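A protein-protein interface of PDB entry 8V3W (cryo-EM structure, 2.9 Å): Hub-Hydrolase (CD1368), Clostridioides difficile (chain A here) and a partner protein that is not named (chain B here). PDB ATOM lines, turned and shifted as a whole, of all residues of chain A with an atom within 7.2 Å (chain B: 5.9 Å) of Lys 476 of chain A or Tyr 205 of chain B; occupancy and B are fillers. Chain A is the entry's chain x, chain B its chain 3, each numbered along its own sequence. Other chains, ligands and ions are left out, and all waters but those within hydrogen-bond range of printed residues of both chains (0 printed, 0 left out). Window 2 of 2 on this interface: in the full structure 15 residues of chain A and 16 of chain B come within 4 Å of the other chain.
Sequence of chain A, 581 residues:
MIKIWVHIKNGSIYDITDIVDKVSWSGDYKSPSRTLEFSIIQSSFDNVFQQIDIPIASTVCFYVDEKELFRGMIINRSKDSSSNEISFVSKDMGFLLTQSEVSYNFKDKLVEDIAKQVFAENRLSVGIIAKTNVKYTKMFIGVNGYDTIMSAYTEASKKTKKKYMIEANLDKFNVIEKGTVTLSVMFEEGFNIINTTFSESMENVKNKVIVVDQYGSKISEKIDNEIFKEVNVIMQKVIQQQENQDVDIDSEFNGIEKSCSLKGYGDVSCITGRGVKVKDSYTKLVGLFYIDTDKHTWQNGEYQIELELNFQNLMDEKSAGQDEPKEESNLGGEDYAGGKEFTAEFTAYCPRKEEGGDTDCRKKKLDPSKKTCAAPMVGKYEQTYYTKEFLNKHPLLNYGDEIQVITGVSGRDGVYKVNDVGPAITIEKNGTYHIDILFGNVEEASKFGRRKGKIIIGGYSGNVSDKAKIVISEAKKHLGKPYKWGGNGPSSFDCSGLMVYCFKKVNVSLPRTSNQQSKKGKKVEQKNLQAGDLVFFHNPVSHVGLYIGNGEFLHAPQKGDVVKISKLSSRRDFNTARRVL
The side-chain amide oxygen (OD1) of Asn 463 of chain A is in hydrogen-bond range of the side-chain hydroxyl (OH) of Tyr 205 of chain B (3.1 Å).
The backbone NH (N) of Tyr 205 of chain B lies within hydrogen-bond range of the backbone carbonyl oxygen (O) of Phe 224 of chain B (2.5 Å).
Gly 203 of chain B touches Lys 469 of chain A (N to NZ, 3.8 Å).
Val 204 of chain B touches Lys 469 of chain A (O to NZ, 3.9 Å).
Ser 473 of chain A touches Leu 199 of chain B (OG to CD1, 3.2 Å).
NZ of Lys 476 of chain A touches O of Tyr 205 of chain B, at 3.7 Å.
Of the printed residues of chain B, Lys 476 of chain A touches Tyr 205 (3.7 Å).
Tyr 205 of chain B touches just these residues of chain A: Asn 463 (3.1 Å) and Lys 476 (3.7 Å).
Of the printed residues of chain A, Leu 199 of chain B touches Ser 473.
Of the printed residues of chain B, Ser 473 of chain A touches Leu 199 (3.2 Å).
Printed residues of chain B within 4 Å of Lys 469 of chain A: Gly 203 and Val 204.
Printed residues of chain A within 4 Å of Val 204 of chain B: Lys 469 (3.9 Å).
Val 563 of chain A touches none of the printed residues of chain B.
Ile 470 of chain A touches none of the printed residues of chain B.
The nearest residue of chain B that does not touch Lys 476 of chain A is Asn 206 of chain B (5.4 Å).
The nearest residue of chain A that does not touch Tyr 205 of chain B is Gly 462 of chain A (4.3 Å).
The nearest printed residue of chain A that does not touch Val 204 of chain B is Asn 463 of chain A (7.1 Å).
Hydrophobic or aromatic side chains of chain B within 4 Å of the printed part of chain A: Leu 199 and Tyr 205.
Of the 23 printed residues of chain A, 4 touch a printed residue of chain B.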
ATOM      1  N   SER A 461      42.152 -24.058 -18.265  1.00  0.00           N
ATOM      2  CA  SER A 461      41.508 -22.889 -18.853  1.00  0.00           C
ATOM      3  C   SER A 461      40.120 -23.209 -19.386  1.00  0.00           C
ATOM      4  O   SER A 461      39.151 -22.524 -19.034  1.00  0.00           O
ATOM      5  CB  SER A 461      42.380 -22.304 -19.974  1.00  0.00           C
ATOM      6  OG  SER A 461      41.863 -21.065 -20.423  1.00  0.00           O
ATOM      7  N   GLY A 462      39.996 -24.237 -20.220  1.00  0.00           N
ATOM      8  CA  GLY A 462      38.698 -24.656 -20.726  1.00  0.00           C
ATOM      9  C   GLY A 462      37.991 -23.621 -21.575  1.00  0.00           C
ATOM     10  O   GLY A 462      36.766 -23.478 -21.482  1.00  0.00           O
ATOM     11  N   ASN A 463      38.735 -22.903 -22.408  1.00  0.00           N
ATOM     12  CA  ASN A 463      38.178 -21.903 -23.306  1.00  0.00           C
ATOM     13  C   ASN A 463      38.198 -22.425 -24.739  1.00  0.00           C
ATOM     14  O   ASN A 463      38.778 -23.470 -25.040  1.00  0.00           O
ATOM     15  CB  ASN A 463      38.952 -20.582 -23.200  1.00  0.00           C
ATOM     16  CG  ASN A 463      38.261 -19.577 -22.297  1.00  0.00           C
ATOM     17  OD1 ASN A 463      37.127 -19.791 -21.868  1.00  0.00           O
ATOM     18  ND2 ASN A 463      38.940 -18.472 -22.007  1.00  0.00           N
ATOM     19  N   VAL A 464      37.535 -21.684 -25.625  1.00  0.00           N
ATOM     20  CA  VAL A 464      37.445 -22.036 -27.042  1.00  0.00           C
ATOM     21  C   VAL A 464      38.206 -21.034 -27.909  1.00  0.00           C
ATOM     22  O   VAL A 464      39.167 -21.394 -28.589  1.00  0.00           O
ATOM     23  CB  VAL A 464      35.973 -22.165 -27.492  1.00  0.00           C
ATOM     24  CG1 VAL A 464      35.888 -22.901 -28.816  1.00  0.00           C
ATOM     25  CG2 VAL A 464      35.155 -22.881 -26.427  1.00  0.00           C
ATOM     26  N   LYS A 469      34.026 -14.766 -26.797  1.00  0.00           N
ATOM     27  CA  LYS A 469      33.540 -13.898 -25.730  1.00  0.00           C
ATOM     28  C   LYS A 469      32.915 -12.626 -26.290  1.00  0.00           C
ATOM     29  O   LYS A 469      31.850 -12.198 -25.833  1.00  0.00           O
ATOM     30  CB  LYS A 469      34.681 -13.554 -24.773  1.00  0.00           C
ATOM     31  CG  LYS A 469      35.085 -14.687 -23.846  1.00  0.00           C
ATOM     32  CD  LYS A 469      36.253 -14.272 -22.963  1.00  0.00           C
ATOM     33  CE  LYS A 469      36.549 -15.315 -21.897  1.00  0.00           C
ATOM     34  NZ  LYS A 469      37.634 -14.868 -20.977  1.00  0.00           N
ATOM     35  N   ILE A 470      33.567 -12.007 -27.276  1.00  0.00           N
ATOM     36  CA  ILE A 470      33.025 -10.798 -27.896  1.00  0.00           C
ATOM     37  C   ILE A 470      31.704 -11.113 -28.583  1.00  0.00           C
ATOM     38  O   ILE A 470      30.722 -10.367 -28.470  1.00  0.00           O
ATOM     39  CB  ILE A 470      34.047 -10.210 -28.884  1.00  0.00           C
ATOM     40  CG1 ILE A 470      35.463 -10.388 -28.337  1.00  0.00           C
ATOM     41  CG2 ILE A 470      33.769  -8.735 -29.124  1.00  0.00           C
ATOM     42  CD1 ILE A 470      36.544 -10.199 -29.372  1.00  0.00           C
ATOM     43  N   VAL A 471      31.669 -12.236 -29.303  1.00  0.00           N
ATOM     44  CA  VAL A 471      30.445 -12.738 -29.922  1.00  0.00           C
ATOM     45  C   VAL A 471      29.313 -12.823 -28.909  1.00  0.00           C
ATOM     46  O   VAL A 471      28.234 -12.236 -29.099  1.00  0.00           O
ATOM     47  CB  VAL A 471      30.746 -14.109 -30.563  1.00  0.00           C
ATOM     48  CG1 VAL A 471      29.497 -14.804 -31.032  1.00  0.00           C
ATOM     49  CG2 VAL A 471      31.663 -13.919 -31.761  1.00  0.00           C
ATOM     50  N   ILE A 472      29.551 -13.525 -27.803  1.00  0.00           N
ATOM     51  CA  ILE A 472      28.492 -13.784 -26.836  1.00  0.00           C
ATOM     52  C   ILE A 472      28.063 -12.491 -26.156  1.00  0.00           C
ATOM     53  O   ILE A 472      26.867 -12.248 -25.955  1.00  0.00           O
ATOM     54  CB  ILE A 472      28.954 -14.853 -25.829  1.00  0.00           C
ATOM     55  CG1 ILE A 472      28.897 -16.238 -26.481  1.00  0.00           C
ATOM     56  CG2 ILE A 472      28.086 -14.841 -24.589  1.00  0.00           C
ATOM     57  CD1 ILE A 472      29.558 -17.326 -25.677  1.00  0.00           C
ATOM     58  N   SER A 473      29.024 -11.634 -25.806  1.00  0.00           N
ATOM     59  CA  SER A 473      28.683 -10.378 -25.149  1.00  0.00           C
ATOM     60  C   SER A 473      27.844  -9.485 -26.052  1.00  0.00           C
ATOM     61  O   SER A 473      26.869  -8.881 -25.597  1.00  0.00           O
ATOM     62  CB  SER A 473      29.948  -9.646 -24.708  1.00  0.00           C
ATOM     63  OG  SER A 473      29.613  -8.489 -23.959  1.00  0.00           O
ATOM     64  N   GLU A 474      28.202  -9.385 -27.335  1.00  0.00           N
ATOM     65  CA  GLU A 474      27.413  -8.573 -28.258  1.00  0.00           C
ATOM     66  C   GLU A 474      26.002  -9.136 -28.406  1.00  0.00           C
ATOM     67  O   GLU A 474      25.007  -8.387 -28.385  1.00  0.00           O
ATOM     68  CB  GLU A 474      28.121  -8.514 -29.613  1.00  0.00           C
ATOM     69  CG  GLU A 474      27.377  -7.767 -30.696  1.00  0.00           C
ATOM     70  CD  GLU A 474      27.366  -6.274 -30.451  1.00  0.00           C
ATOM     71  OE1 GLU A 474      28.219  -5.792 -29.675  1.00  0.00           O
ATOM     72  OE2 GLU A 474      26.517  -5.582 -31.038  1.00  0.00           O
ATOM     73  N   ALA A 475      25.896 -10.463 -28.521  1.00  0.00           N
ATOM     74  CA  ALA A 475      24.584 -11.086 -28.642  1.00  0.00           C
ATOM     75  C   ALA A 475      23.728 -10.810 -27.411  1.00  0.00           C
ATOM     76  O   ALA A 475      22.520 -10.572 -27.528  1.00  0.00           O
ATOM     77  CB  ALA A 475      24.739 -12.586 -28.876  1.00  0.00           C
ATOM     78  N   LYS A 476      24.335 -10.839 -26.221  1.00  0.00           N
ATOM     79  CA  LYS A 476      23.606 -10.434 -25.022  1.00  0.00           C
ATOM     80  C   LYS A 476      23.270  -8.948 -25.049  1.00  0.00           C
ATOM     81  O   LYS A 476      22.242  -8.535 -24.500  1.00  0.00           O
ATOM     82  CB  LYS A 476      24.411 -10.760 -23.762  1.00  0.00           C
ATOM     83  CG  LYS A 476      24.816 -12.214 -23.623  1.00  0.00           C
ATOM     84  CD  LYS A 476      26.158 -12.338 -22.919  1.00  0.00           C
ATOM     85  CE  LYS A 476      26.092 -13.307 -21.753  1.00  0.00           C
ATOM     86  NZ  LYS A 476      27.418 -13.933 -21.485  1.00  0.00           N
ATOM     87  N   LYS A 477      24.127  -8.135 -25.669  1.00  0.00           N
ATOM     88  CA  LYS A 477      23.858  -6.705 -25.764  1.00  0.00           C
ATOM     89  C   LYS A 477      22.596  -6.432 -26.564  1.00  0.00           C
ATOM     90  O   LYS A 477      21.904  -5.440 -26.311  1.00  0.00           O
ATOM     91  CB  LYS A 477      25.041  -5.979 -26.405  1.00  0.00           C
ATOM     92  CG  LYS A 477      26.260  -5.813 -25.520  1.00  0.00           C
ATOM     93  CD  LYS A 477      27.402  -5.195 -26.312  1.00  0.00           C
ATOM     94  CE  LYS A 477      28.705  -5.221 -25.536  1.00  0.00           C
ATOM     95  NZ  LYS A 477      29.842  -4.727 -26.359  1.00  0.00           N
ATOM     96  N   HIS A 478      22.275  -7.297 -27.523  1.00  0.00           N
ATOM     97  CA  HIS A 478      21.055  -7.122 -28.307  1.00  0.00           C
ATOM     98  C   HIS A 478      19.847  -7.877 -27.758  1.00  0.00           C
ATOM     99  O   HIS A 478      18.892  -8.108 -28.504  1.00  0.00           O
ATOM    100  CB  HIS A 478      21.291  -7.515 -29.764  1.00  0.00           C
ATOM    101  CG  HIS A 478      22.459  -6.824 -30.392  1.00  0.00           C
ATOM    102  ND1 HIS A 478      22.598  -5.453 -30.375  1.00  0.00           N
ATOM    103  CD2 HIS A 478      23.526  -7.303 -31.075  1.00  0.00           C
ATOM    104  CE1 HIS A 478      23.704  -5.117 -31.012  1.00  0.00           C
ATOM    105  NE2 HIS A 478      24.287  -6.221 -31.444  1.00  0.00           N
ATOM    106  N   LEU A 479      19.854  -8.254 -26.482  1.00  0.00           N
ATOM    107  CA  LEU A 479      18.706  -8.946 -25.909  1.00  0.00           C
ATOM    108  C   LEU A 479      17.500  -8.020 -25.782  1.00  0.00           C
ATOM    109  O   LEU A 479      17.629  -6.851 -25.409  1.00  0.00           O
ATOM    110  CB  LEU A 479      19.059  -9.521 -24.538  1.00  0.00           C
ATOM    111  CG  LEU A 479      19.939 -10.769 -24.560  1.00  0.00           C
ATOM    112  CD1 LEU A 479      20.405 -11.123 -23.160  1.00  0.00           C
ATOM    113  CD2 LEU A 479      19.216 -11.935 -25.211  1.00  0.00           C
ATOM    114  N   GLY A 480      16.320  -8.557 -26.092  1.00  0.00           N
ATOM    115  CA  GLY A 480      15.065  -7.886 -25.818  1.00  0.00           C
ATOM    116  C   GLY A 480      14.634  -6.846 -26.826  1.00  0.00           C
ATOM    117  O   GLY A 480      13.572  -6.237 -26.643  1.00  0.00           O
ATOM    118  N   LEU A 498      21.308 -10.793 -36.489  1.00  0.00           N
ATOM    119  CA  LEU A 498      21.982 -10.780 -35.196  1.00  0.00           C
ATOM    120  C   LEU A 498      23.405 -11.304 -35.323  1.00  0.00           C
ATOM    121  O   LEU A 498      24.367 -10.610 -34.976  1.00  0.00           O
ATOM    122  CB  LEU A 498      21.185 -11.618 -34.190  1.00  0.00           C
ATOM    123  CG  LEU A 498      21.317 -11.389 -32.679  1.00  0.00           C
ATOM    124  CD1 LEU A 498      20.309 -12.254 -31.945  1.00  0.00           C
ATOM    125  CD2 LEU A 498      22.723 -11.675 -32.159  1.00  0.00           C
ATOM    126  N   ALA A 531      30.437 -23.124 -26.943  1.00  0.00           N
ATOM    127  CA  ALA A 531      30.038 -21.724 -26.947  1.00  0.00           C
ATOM    128  C   ALA A 531      30.467 -21.054 -28.245  1.00  0.00           C
ATOM    129  O   ALA A 531      31.618 -21.175 -28.670  1.00  0.00           O
ATOM    130  CB  ALA A 531      30.645 -20.997 -25.748  1.00  0.00           C
ATOM    131  N   LEU A 546      22.483 -18.734 -31.890  1.00  0.00           N
ATOM    132  CA  LEU A 546      23.898 -18.705 -31.540  1.00  0.00           C
ATOM    133  C   LEU A 546      24.073 -19.486 -30.243  1.00  0.00           C
ATOM    134  O   LEU A 546      23.624 -19.042 -29.181  1.00  0.00           O
ATOM    135  CB  LEU A 546      24.394 -17.269 -31.394  1.00  0.00           C
ATOM    136  CG  LEU A 546      25.742 -17.075 -30.695  1.00  0.00           C
ATOM    137  CD1 LEU A 546      26.858 -17.763 -31.461  1.00  0.00           C
ATOM    138  CD2 LEU A 546      26.033 -15.594 -30.533  1.00  0.00           C
ATOM    139  N   ILE A 548      25.485 -20.815 -26.957  1.00  0.00           N
ATOM    140  CA  ILE A 548      26.364 -20.292 -25.918  1.00  0.00           C
ATOM    141  C   ILE A 548      26.729 -21.362 -24.900  1.00  0.00           C
ATOM    142  O   ILE A 548      27.340 -21.053 -23.873  1.00  0.00           O
ATOM    143  CB  ILE A 548      25.743 -19.074 -25.217  1.00  0.00           C
ATOM    144  CG1 ILE A 548      24.545 -19.506 -24.369  1.00  0.00           C
ATOM    145  CG2 ILE A 548      25.319 -18.032 -26.242  1.00  0.00           C
ATOM    146  CD1 ILE A 548      24.037 -18.429 -23.441  1.00  0.00           C
ATOM    147  N   LEU A 554      21.231 -17.970 -28.079  1.00  0.00           N
ATOM    148  CA  LEU A 554      20.604 -16.679 -28.323  1.00  0.00           C
ATOM    149  C   LEU A 554      20.174 -16.572 -29.779  1.00  0.00           C
ATOM    150  O   LEU A 554      20.849 -17.086 -30.678  1.00  0.00           O
ATOM    151  CB  LEU A 554      21.542 -15.516 -27.975  1.00  0.00           C
ATOM    152  CG  LEU A 554      21.710 -15.123 -26.500  1.00  0.00           C
ATOM    153  CD1 LEU A 554      22.105 -16.302 -25.629  1.00  0.00           C
ATOM    154  CD2 LEU A 554      22.706 -13.990 -26.341  1.00  0.00           C
ATOM    155  N   VAL A 563      14.451 -10.525 -28.788  1.00  0.00           N
ATOM    156  CA  VAL A 563      15.652 -11.328 -28.603  1.00  0.00           C
ATOM    157  C   VAL A 563      15.747 -11.783 -27.156  1.00  0.00           C
ATOM    158  O   VAL A 563      15.636 -10.978 -26.222  1.00  0.00           O
ATOM    159  CB  VAL A 563      16.894 -10.530 -29.024  1.00  0.00           C
ATOM    160  CG1 VAL A 563      18.131 -11.412 -28.989  1.00  0.00           C
ATOM    161  CG2 VAL A 563      16.691  -9.927 -30.406  1.00  0.00           C
ATOM    162  N   ILE A 565      16.861 -15.683 -24.611  1.00  0.00           N
ATOM    163  CA  ILE A 565      17.651 -16.901 -24.497  1.00  0.00           C
ATOM    164  C   ILE A 565      16.691 -18.079 -24.461  1.00  0.00           C
ATOM    165  O   ILE A 565      15.719 -18.070 -23.695  1.00  0.00           O
ATOM    166  CB  ILE A 565      18.548 -16.884 -23.247  1.00  0.00           C
ATOM    167  CG1 ILE A 565      19.515 -15.702 -23.308  1.00  0.00           C
ATOM    168  CG2 ILE A 565      19.315 -18.191 -23.124  1.00  0.00           C
ATOM    169  CD1 ILE A 565      20.357 -15.537 -22.068  1.00  0.00           C
ATOM    170  N   LEU B 199      35.355  -7.689 -19.189  1.00  0.00           N
ATOM    171  CA  LEU B 199      35.385  -8.862 -20.054  1.00  0.00           C
ATOM    172  C   LEU B 199      36.769  -9.104 -20.646  1.00  0.00           C
ATOM    173  O   LEU B 199      37.115 -10.252 -20.950  1.00  0.00           O
ATOM    174  CB  LEU B 199      34.353  -8.713 -21.168  1.00  0.00           C
ATOM    175  CG  LEU B 199      32.903  -8.846 -20.707  1.00  0.00           C
ATOM    176  CD1 LEU B 199      31.961  -8.501 -21.843  1.00  0.00           C
ATOM    177  CD2 LEU B 199      32.630 -10.241 -20.168  1.00  0.00           C
ATOM    178  N   GLY B 203      38.947 -15.499 -17.469  1.00  0.00           N
ATOM    179  CA  GLY B 203      38.321 -16.112 -16.317  1.00  0.00           C
ATOM    180  C   GLY B 203      37.020 -15.479 -15.880  1.00  0.00           C
ATOM    181  O   GLY B 203      36.477 -15.872 -14.842  1.00  0.00           O
ATOM    182  N   VAL B 204      36.500 -14.518 -16.639  1.00  0.00           N
ATOM    183  CA  VAL B 204      35.267 -13.818 -16.305  1.00  0.00           C
ATOM    184  C   VAL B 204      34.261 -14.053 -17.421  1.00  0.00           C
ATOM    185  O   VAL B 204      34.610 -13.993 -18.605  1.00  0.00           O
ATOM    186  CB  VAL B 204      35.514 -12.311 -16.093  1.00  0.00           C
ATOM    187  CG1 VAL B 204      34.213 -11.600 -15.762  1.00  0.00           C
ATOM    188  CG2 VAL B 204      36.539 -12.098 -14.987  1.00  0.00           C
ATOM    189  N   TYR B 205      33.015 -14.326 -17.041  1.00  0.00           N
ATOM    190  CA  TYR B 205      31.968 -14.659 -17.996  1.00  0.00           C
ATOM    191  C   TYR B 205      30.759 -13.735 -17.940  1.00  0.00           C
ATOM    192  O   TYR B 205      30.144 -13.494 -18.981  1.00  0.00           O
ATOM    193  CB  TYR B 205      31.504 -16.109 -17.787  1.00  0.00           C
ATOM    194  CG  TYR B 205      32.523 -17.144 -18.222  1.00  0.00           C
ATOM    195  CD1 TYR B 205      33.700 -17.333 -17.507  1.00  0.00           C
ATOM    196  CD2 TYR B 205      32.307 -17.932 -19.346  1.00  0.00           C
ATOM    197  CE1 TYR B 205      34.633 -18.271 -17.899  1.00  0.00           C
ATOM    198  CE2 TYR B 205      33.237 -18.877 -19.746  1.00  0.00           C
ATOM    199  CZ  TYR B 205      34.397 -19.042 -19.018  1.00  0.00           C
ATOM    200  OH  TYR B 205      35.327 -19.979 -19.408  1.00  0.00           O
ATOM    201  N   ASN B 206      30.402 -13.212 -16.768  1.00  0.00           N
ATOM    202  CA  ASN B 206      29.289 -12.281 -16.642  1.00  0.00           C
ATOM    203  C   ASN B 206      29.718 -11.119 -15.760  1.00  0.00           C
ATOM    204  O   ASN B 206      30.460 -11.309 -14.792  1.00  0.00           O
ATOM    205  CB  ASN B 206      28.045 -12.966 -16.060  1.00  0.00           C
ATOM    206  CG  ASN B 206      26.992 -11.978 -15.597  1.00  0.00           C
ATOM    207  OD1 ASN B 206      26.774 -10.943 -16.226  1.00  0.00           O
ATOM    208  ND2 ASN B 206      26.331 -12.295 -14.490  1.00  0.00           N
ATOM    209  N   VAL B 207      29.258  -9.916 -16.101  1.00  0.00           N
ATOM    210  CA  VAL B 207      29.705  -8.694 -15.442  1.00  0.00           C
ATOM    211  C   VAL B 207      28.500  -7.824 -15.115  1.00  0.00           C
ATOM    212  O   VAL B 207      27.663  -7.559 -15.986  1.00  0.00           O
ATOM    213  CB  VAL B 207      30.708  -7.920 -16.317  1.00  0.00           C
ATOM    214  CG1 VAL B 207      31.026  -6.565 -15.695  1.00  0.00           C
ATOM    215  CG2 VAL B 207      31.969  -8.740 -16.521  1.00  0.00           C
ATOM    216  N   PHE B 224      31.712 -12.467 -12.883  1.00  0.00           N
ATOM    217  CA  PHE B 224      31.218 -13.825 -12.705  1.00  0.00           C
ATOM    218  C   PHE B 224      32.050 -14.794 -13.529  1.00  0.00           C
ATOM    219  O   PHE B 224      32.416 -14.498 -14.671  1.00  0.00           O
ATOM    220  CB  PHE B 224      29.744 -13.947 -13.107  1.00  0.00           C
ATOM    221  CG  PHE B 224      28.799 -13.246 -12.176  1.00  0.00           C
ATOM    222  CD1 PHE B 224      28.600 -11.879 -12.270  1.00  0.00           C
ATOM    223  CD2 PHE B 224      28.109 -13.955 -11.207  1.00  0.00           C
ATOM    224  CE1 PHE B 224      27.729 -11.231 -11.415  1.00  0.00           C
ATOM    225  CE2 PHE B 224      27.237 -13.314 -10.349  1.00  0.00           C
ATOM    226  CZ  PHE B 224      27.047 -11.950 -10.454  1.00  0.00           C
ATOM    227  N   GLY B 225      32.341 -15.950 -12.947  1.00  0.00           N
ATOM    228  CA  GLY B 225      33.087 -16.994 -13.615  1.00  0.00           C
ATOM    229  C   GLY B 225      32.198 -17.899 -14.440  1.00  0.00           C
ATOM    230  O   GLY B 225      31.064 -17.556 -14.788  1.00  0.00           O
ATOM    231  N   LYS B 226      32.734 -19.073 -14.766  1.00  0.00           N
ATOM    232  CA  LYS B 226      31.975 -20.055 -15.528  1.00  0.00           C
ATOM    233  C   LYS B 226      30.723 -20.463 -14.764  1.00  0.00           C
ATOM    234  O   LYS B 226      30.783 -20.772 -13.570  1.00  0.00           O
ATOM    235  CB  LYS B 226      32.840 -21.280 -15.820  1.00  0.00           C
ATOM    236  CG  LYS B 226      32.263 -22.208 -16.872  1.00  0.00           C
ATOM    237  CD  LYS B 226      33.293 -23.229 -17.326  1.00  0.00           C
ATOM    238  CE  LYS B 226      32.763 -24.079 -18.467  1.00  0.00           C
ATOM    239  NZ  LYS B 226      33.792 -25.030 -18.969  1.00  0.00           N
ATOM    240  N   ASN B 227      29.587 -20.467 -15.466  1.00  0.00           N
ATOM    241  CA  ASN B 227      28.280 -20.734 -14.863  1.00  0.00           C
ATOM    242  C   ASN B 227      27.994 -19.766 -13.718  1.00  0.00           C
ATOM    243  O   ASN B 227      27.364 -20.125 -12.720  1.00  0.00           O
ATOM    244  CB  ASN B 227      28.167 -22.186 -14.394  1.00  0.00           C
ATOM    245  CG  ASN B 227      28.982 -23.135 -15.243  1.00  0.00           C
ATOM    246  OD1 ASN B 227      28.681 -23.349 -16.418  1.00  0.00           O
ATOM    247  ND2 ASN B 227      30.031 -23.701 -14.657  1.00  0.00           N
ATOM    248  N   ASN B 228      28.463 -18.527 -13.872  1.00  0.00           N
ATOM    249  CA  ASN B 228      28.213 -17.450 -12.913  1.00  0.00           C
ATOM    250  C   ASN B 228      28.648 -17.848 -11.505  1.00  0.00           C
ATOM    251  O   ASN B 228      27.971 -17.563 -10.515  1.00  0.00           O
ATOM    252  CB  ASN B 228      26.741 -17.034 -12.939  1.00  0.00           C
ATOM    253  CG  ASN B 228      26.331 -16.433 -14.271  1.00  0.00           C
ATOM    254  OD1 ASN B 228      27.151 -15.850 -14.979  1.00  0.00           O
ATOM    255  ND2 ASN B 228      25.056 -16.573 -14.618  1.00  0.00           N
